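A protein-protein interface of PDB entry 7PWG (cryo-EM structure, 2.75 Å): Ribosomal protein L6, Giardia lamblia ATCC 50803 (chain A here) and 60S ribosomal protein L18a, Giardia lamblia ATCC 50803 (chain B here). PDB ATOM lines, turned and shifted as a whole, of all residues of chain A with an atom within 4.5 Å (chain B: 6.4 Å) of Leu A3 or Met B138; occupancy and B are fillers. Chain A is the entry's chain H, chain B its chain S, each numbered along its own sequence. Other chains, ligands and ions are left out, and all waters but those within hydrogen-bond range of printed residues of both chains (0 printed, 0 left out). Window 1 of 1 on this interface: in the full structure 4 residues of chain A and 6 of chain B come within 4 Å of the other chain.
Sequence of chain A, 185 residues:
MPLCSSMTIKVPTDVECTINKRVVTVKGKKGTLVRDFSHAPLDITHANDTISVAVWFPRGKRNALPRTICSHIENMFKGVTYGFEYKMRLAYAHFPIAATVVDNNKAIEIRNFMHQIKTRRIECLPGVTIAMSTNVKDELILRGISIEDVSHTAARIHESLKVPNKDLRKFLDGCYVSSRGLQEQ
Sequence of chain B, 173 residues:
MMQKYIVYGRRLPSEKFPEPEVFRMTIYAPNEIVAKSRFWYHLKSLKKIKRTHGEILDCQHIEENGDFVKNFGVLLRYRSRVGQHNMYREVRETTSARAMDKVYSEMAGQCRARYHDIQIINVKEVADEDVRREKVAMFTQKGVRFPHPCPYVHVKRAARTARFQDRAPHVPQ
N of Pro A2 lies close to OE1 of Glu B134 (3.3 Å). The backbone nitrogen (N) of Pro A2 lies close to the side-chain sulfur (SD) of Met B138, at 3.7 Å.
The backbone NH (N) of Phe A57 sits at hydrogen-bond distance from the backbone carbonyl oxygen (O) of Leu A3 (2.9 Å).
CE of Met B138 touches CG of Leu A3, at 3.6 Å. Val B144 touches Leu A3 (CG2 to CD1, 3.6 Å). O of Arg B145 touches CZ3 of Trp A56 (3.9 Å).
Printed residues of chain B within 4 Å of Pro A2: Glu B134 (3.3 Å) and Met B138 (3.7 Å). Leu A3 touches just these residues of chain B: Met B138 (3.6 Å) and Val B144 (3.6 Å). Pro A58 touches none of the printed residues of chain B. Of the printed residues of chain A, Glu B134 touches Pro A2. Val B136 touches none of the printed residues of chain A. Met B138 touches just these residues of chain A: Pro A2 (3.7 Å) and Leu A3 (3.6 Å). The nearest residue of chain B that does not touch Leu A3 is Phe B146 (4.2 Å). The nearest printed residue of chain A that does not touch Met B138 is Cys A4 (6.9 Å).
Hydrophobic or aromatic side chains of chain B that line the printed part of chain A: Met B138 and Val B144. Among the printed residues, no Asp or Glu carboxylate lies within 4 Å of a Lys or Arg side-chain nitrogen of the other chain.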
ATOM      1  N   PRO A   2     -16.657  11.343  15.810  1.00  0.00           N
ATOM      2  CA  PRO A   2     -15.917  11.501  17.060  1.00  0.00           C
ATOM      3  C   PRO A   2     -16.503  12.593  17.919  1.00  0.00           C
ATOM      4  O   PRO A   2     -17.336  13.349  17.436  1.00  0.00           O
ATOM      5  CB  PRO A   2     -14.510  11.868  16.587  1.00  0.00           C
ATOM      6  CG  PRO A   2     -14.399  11.259  15.274  1.00  0.00           C
ATOM      7  CD  PRO A   2     -15.760  11.390  14.644  1.00  0.00           C
ATOM      8  N   LEU A   3     -16.087  12.656  19.181  1.00  0.00           N
ATOM      9  CA  LEU A   3     -16.518  13.714  20.083  1.00  0.00           C
ATOM     10  C   LEU A   3     -15.590  14.918  20.060  1.00  0.00           C
ATOM     11  O   LEU A   3     -16.019  16.022  20.406  1.00  0.00           O
ATOM     12  CB  LEU A   3     -16.608  13.178  21.510  1.00  0.00           C
ATOM     13  CG  LEU A   3     -17.652  12.100  21.777  1.00  0.00           C
ATOM     14  CD1 LEU A   3     -17.289  11.335  23.012  1.00  0.00           C
ATOM     15  CD2 LEU A   3     -19.026  12.715  21.927  1.00  0.00           C
ATOM     16  N   CYS A   4     -14.331  14.722  19.682  1.00  0.00           N
ATOM     17  CA  CYS A   4     -13.352  15.792  19.655  1.00  0.00           C
ATOM     18  C   CYS A   4     -12.406  15.567  18.488  1.00  0.00           C
ATOM     19  O   CYS A   4     -12.031  14.433  18.197  1.00  0.00           O
ATOM     20  CB  CYS A   4     -12.561  15.851  20.962  1.00  0.00           C
ATOM     21  SG  CYS A   4     -11.837  17.458  21.308  1.00  0.00           S
ATOM     22  N   VAL A  55     -11.736  20.911  19.023  1.00  0.00           N
ATOM     23  CA  VAL A  55     -13.116  21.318  18.801  1.00  0.00           C
ATOM     24  C   VAL A  55     -14.027  20.191  19.258  1.00  0.00           C
ATOM     25  O   VAL A  55     -13.965  19.086  18.720  1.00  0.00           O
ATOM     26  CB  VAL A  55     -13.392  21.678  17.331  1.00  0.00           C
ATOM     27  CG1 VAL A  55     -14.815  22.154  17.173  1.00  0.00           C
ATOM     28  CG2 VAL A  55     -12.463  22.763  16.871  1.00  0.00           C
ATOM     29  N   TRP A  56     -14.887  20.473  20.227  1.00  0.00           N
ATOM     30  CA  TRP A  56     -15.842  19.494  20.721  1.00  0.00           C
ATOM     31  C   TRP A  56     -17.111  19.505  19.889  1.00  0.00           C
ATOM     32  O   TRP A  56     -17.643  20.565  19.567  1.00  0.00           O
ATOM     33  CB  TRP A  56     -16.193  19.761  22.178  1.00  0.00           C
ATOM     34  CG  TRP A  56     -15.077  19.561  23.132  1.00  0.00           C
ATOM     35  CD1 TRP A  56     -14.247  20.509  23.613  1.00  0.00           C
ATOM     36  CD2 TRP A  56     -14.678  18.333  23.738  1.00  0.00           C
ATOM     37  NE1 TRP A  56     -13.352  19.959  24.487  1.00  0.00           N
ATOM     38  CE2 TRP A  56     -13.598  18.619  24.581  1.00  0.00           C
ATOM     39  CE3 TRP A  56     -15.127  17.021  23.645  1.00  0.00           C
ATOM     40  CZ2 TRP A  56     -12.967  17.647  25.326  1.00  0.00           C
ATOM     41  CZ3 TRP A  56     -14.509  16.070  24.378  1.00  0.00           C
ATOM     42  CH2 TRP A  56     -13.437  16.380  25.213  1.00  0.00           C
ATOM     43  N   PHE A  57     -17.598  18.312  19.569  1.00  0.00           N
ATOM     44  CA  PHE A  57     -18.728  18.005  18.701  1.00  0.00           C
ATOM     45  C   PHE A  57     -18.595  18.724  17.368  1.00  0.00           C
ATOM     46  O   PHE A  57     -19.351  19.662  17.097  1.00  0.00           O
ATOM     47  CB  PHE A  57     -20.069  18.375  19.340  1.00  0.00           C
ATOM     48  CG  PHE A  57     -20.105  18.235  20.836  1.00  0.00           C
ATOM     49  CD1 PHE A  57     -20.193  17.001  21.436  1.00  0.00           C
ATOM     50  CD2 PHE A  57     -20.064  19.352  21.636  1.00  0.00           C
ATOM     51  CE1 PHE A  57     -20.235  16.895  22.800  1.00  0.00           C
ATOM     52  CE2 PHE A  57     -20.090  19.251  22.992  1.00  0.00           C
ATOM     53  CZ  PHE A  57     -20.173  18.023  23.576  1.00  0.00           C
ATOM     54  N   PRO A  58     -17.651  18.329  16.519  1.00  0.00           N
ATOM     55  CA  PRO A  58     -17.585  18.918  15.187  1.00  0.00           C
ATOM     56  C   PRO A  58     -18.611  18.258  14.286  1.00  0.00           C
ATOM     57  O   PRO A  58     -18.837  17.050  14.356  1.00  0.00           O
ATOM     58  CB  PRO A  58     -16.154  18.600  14.749  1.00  0.00           C
ATOM     59  CG  PRO A  58     -15.877  17.317  15.398  1.00  0.00           C
ATOM     60  CD  PRO A  58     -16.589  17.323  16.709  1.00  0.00           C
ATOM     61  N   ARG B 133     -21.258   1.032  13.466  1.00  0.00           N
ATOM     62  CA  ARG B 133     -21.555   2.433  13.184  1.00  0.00           C
ATOM     63  C   ARG B 133     -20.798   3.341  14.148  1.00  0.00           C
ATOM     64  O   ARG B 133     -20.722   3.064  15.348  1.00  0.00           O
ATOM     65  CB  ARG B 133     -23.060   2.717  13.263  1.00  0.00           C
ATOM     66  CG  ARG B 133     -23.928   1.950  12.264  1.00  0.00           C
ATOM     67  CD  ARG B 133     -24.074   2.681  10.940  1.00  0.00           C
ATOM     68  NE  ARG B 133     -25.048   2.038  10.069  1.00  0.00           N
ATOM     69  CZ  ARG B 133     -24.747   1.372   8.962  1.00  0.00           C
ATOM     70  NH1 ARG B 133     -23.490   1.267   8.562  1.00  0.00           N
ATOM     71  NH2 ARG B 133     -25.707   0.818   8.250  1.00  0.00           N
ATOM     72  N   GLU B 134     -20.234   4.428  13.617  1.00  0.00           N
ATOM     73  CA  GLU B 134     -19.323   5.258  14.399  1.00  0.00           C
ATOM     74  C   GLU B 134     -20.027   5.912  15.573  1.00  0.00           C
ATOM     75  O   GLU B 134     -19.481   5.963  16.680  1.00  0.00           O
ATOM     76  CB  GLU B 134     -18.687   6.326  13.513  1.00  0.00           C
ATOM     77  CG  GLU B 134     -17.205   6.548  13.756  1.00  0.00           C
ATOM     78  CD  GLU B 134     -16.909   7.486  14.908  1.00  0.00           C
ATOM     79  OE1 GLU B 134     -17.805   8.263  15.301  1.00  0.00           O
ATOM     80  OE2 GLU B 134     -15.770   7.448  15.419  1.00  0.00           O
ATOM     81  N   LYS B 135     -21.241   6.415  15.351  1.00  0.00           N
ATOM     82  CA  LYS B 135     -21.947   7.161  16.384  1.00  0.00           C
ATOM     83  C   LYS B 135     -22.170   6.305  17.624  1.00  0.00           C
ATOM     84  O   LYS B 135     -21.848   6.717  18.741  1.00  0.00           O
ATOM     85  CB  LYS B 135     -23.271   7.661  15.824  1.00  0.00           C
ATOM     86  CG  LYS B 135     -23.720   8.989  16.336  1.00  0.00           C
ATOM     87  CD  LYS B 135     -25.045   9.384  15.700  1.00  0.00           C
ATOM     88  CE  LYS B 135     -24.865   9.846  14.276  1.00  0.00           C
ATOM     89  NZ  LYS B 135     -24.037  11.065  14.171  1.00  0.00           N
ATOM     90  N   VAL B 136     -22.700   5.097  17.436  1.00  0.00           N
ATOM     91  CA  VAL B 136     -22.908   4.174  18.544  1.00  0.00           C
ATOM     92  C   VAL B 136     -21.580   3.811  19.192  1.00  0.00           C
ATOM     93  O   VAL B 136     -21.418   3.917  20.410  1.00  0.00           O
ATOM     94  CB  VAL B 136     -23.650   2.920  18.044  1.00  0.00           C
ATOM     95  CG1 VAL B 136     -23.728   1.863  19.121  1.00  0.00           C
ATOM     96  CG2 VAL B 136     -25.020   3.284  17.536  1.00  0.00           C
ATOM     97  N   ALA B 137     -20.590   3.445  18.374  1.00  0.00           N
ATOM     98  CA  ALA B 137     -19.331   2.893  18.874  1.00  0.00           C
ATOM     99  C   ALA B 137     -18.608   3.830  19.834  1.00  0.00           C
ATOM    100  O   ALA B 137     -17.938   3.359  20.756  1.00  0.00           O
ATOM    101  CB  ALA B 137     -18.414   2.551  17.705  1.00  0.00           C
ATOM    102  N   MET B 138     -18.717   5.146  19.633  1.00  0.00           N
ATOM    103  CA  MET B 138     -18.050   6.099  20.515  1.00  0.00           C
ATOM    104  C   MET B 138     -18.378   5.835  21.978  1.00  0.00           C
ATOM    105  O   MET B 138     -17.516   5.964  22.850  1.00  0.00           O
ATOM    106  CB  MET B 138     -18.458   7.526  20.153  1.00  0.00           C
ATOM    107  CG  MET B 138     -17.744   8.118  18.966  1.00  0.00           C
ATOM    108  SD  MET B 138     -18.745   9.324  18.070  1.00  0.00           S
ATOM    109  CE  MET B 138     -19.521  10.197  19.402  1.00  0.00           C
ATOM    110  N   PHE B 139     -19.621   5.470  22.264  1.00  0.00           N
ATOM    111  CA  PHE B 139     -20.086   5.326  23.628  1.00  0.00           C
ATOM    112  C   PHE B 139     -19.959   3.905  24.158  1.00  0.00           C
ATOM    113  O   PHE B 139     -20.206   3.683  25.346  1.00  0.00           O
ATOM    114  CB  PHE B 139     -21.534   5.807  23.724  1.00  0.00           C
ATOM    115  CG  PHE B 139     -21.743   7.196  23.205  1.00  0.00           C
ATOM    116  CD1 PHE B 139     -22.047   7.419  21.874  1.00  0.00           C
ATOM    117  CD2 PHE B 139     -21.636   8.283  24.046  1.00  0.00           C
ATOM    118  CE1 PHE B 139     -22.235   8.694  21.405  1.00  0.00           C
ATOM    119  CE2 PHE B 139     -21.819   9.557  23.579  1.00  0.00           C
ATOM    120  CZ  PHE B 139     -22.119   9.766  22.266  1.00  0.00           C
ATOM    121  N   THR B 140     -19.557   2.950  23.324  1.00  0.00           N
ATOM    122  CA  THR B 140     -19.274   1.581  23.753  1.00  0.00           C
ATOM    123  C   THR B 140     -17.840   1.453  24.256  1.00  0.00           C
ATOM    124  O   THR B 140     -17.084   0.595  23.816  1.00  0.00           O
ATOM    125  CB  THR B 140     -19.533   0.593  22.617  1.00  0.00           C
ATOM    126  OG1 THR B 140     -18.568   0.778  21.578  1.00  0.00           O
ATOM    127  CG2 THR B 140     -20.912   0.771  22.027  1.00  0.00           C
ATOM    128  N   GLN B 141     -17.451   2.310  25.197  1.00  0.00           N
ATOM    129  CA  GLN B 141     -16.064   2.399  25.627  1.00  0.00           C
ATOM    130  C   GLN B 141     -16.011   2.557  27.137  1.00  0.00           C
ATOM    131  O   GLN B 141     -17.038   2.673  27.814  1.00  0.00           O
ATOM    132  CB  GLN B 141     -15.347   3.568  24.941  1.00  0.00           C
ATOM    133  N   VAL B 144     -15.722   7.436  28.745  1.00  0.00           N
ATOM    134  CA  VAL B 144     -16.084   8.498  27.815  1.00  0.00           C
ATOM    135  C   VAL B 144     -16.506   9.741  28.594  1.00  0.00           C
ATOM    136  O   VAL B 144     -17.321   9.670  29.521  1.00  0.00           O
ATOM    137  CB  VAL B 144     -17.172   8.013  26.839  1.00  0.00           C
ATOM    138  CG1 VAL B 144     -18.497   7.822  27.516  1.00  0.00           C
ATOM    139  CG2 VAL B 144     -17.319   8.966  25.671  1.00  0.00           C
ATOM    140  N   ARG B 145     -15.907  10.880  28.258  1.00  0.00           N
ATOM    141  CA  ARG B 145     -16.248  12.164  28.855  1.00  0.00           C
ATOM    142  C   ARG B 145     -16.425  13.198  27.765  1.00  0.00           C
ATOM    143  O   ARG B 145     -15.674  13.222  26.787  1.00  0.00           O
ATOM    144  CB  ARG B 145     -15.188  12.697  29.804  1.00  0.00           C
ATOM    145  CG  ARG B 145     -14.413  11.680  30.571  1.00  0.00           C
ATOM    146  CD  ARG B 145     -13.965  12.282  31.897  1.00  0.00           C
ATOM    147  NE  ARG B 145     -12.922  13.286  31.727  1.00  0.00           N
ATOM    148  CZ  ARG B 145     -12.781  14.353  32.505  1.00  0.00           C
ATOM    149  NH1 ARG B 145     -13.632  14.563  33.497  1.00  0.00           N
ATOM    150  NH2 ARG B 145     -11.807  15.217  32.282  1.00  0.00           N
ATOM    151  N   PHE B 146     -17.410  14.061  27.946  1.00  0.00           N
ATOM    152  CA  PHE B 146     -17.546  15.241  27.116  1.00  0.00           C
ATOM    153  C   PHE B 146     -18.138  16.345  27.966  1.00  0.00           C
ATOM    154  O   PHE B 146     -18.751  16.074  29.002  1.00  0.00           O
ATOM    155  CB  PHE B 146     -18.405  14.978  25.872  1.00  0.00           C
ATOM    156  CG  PHE B 146     -19.639  14.163  26.125  1.00  0.00           C
ATOM    157  CD1 PHE B 146     -19.573  12.788  26.179  1.00  0.00           C
ATOM    158  CD2 PHE B 146     -20.871  14.773  26.259  1.00  0.00           C
ATOM    159  CE1 PHE B 146     -20.700  12.041  26.396  1.00  0.00           C
ATOM    160  CE2 PHE B 146     -22.006  14.018  26.481  1.00  0.00           C
ATOM    161  CZ  PHE B 146     -21.919  12.656  26.543  1.00  0.00           C
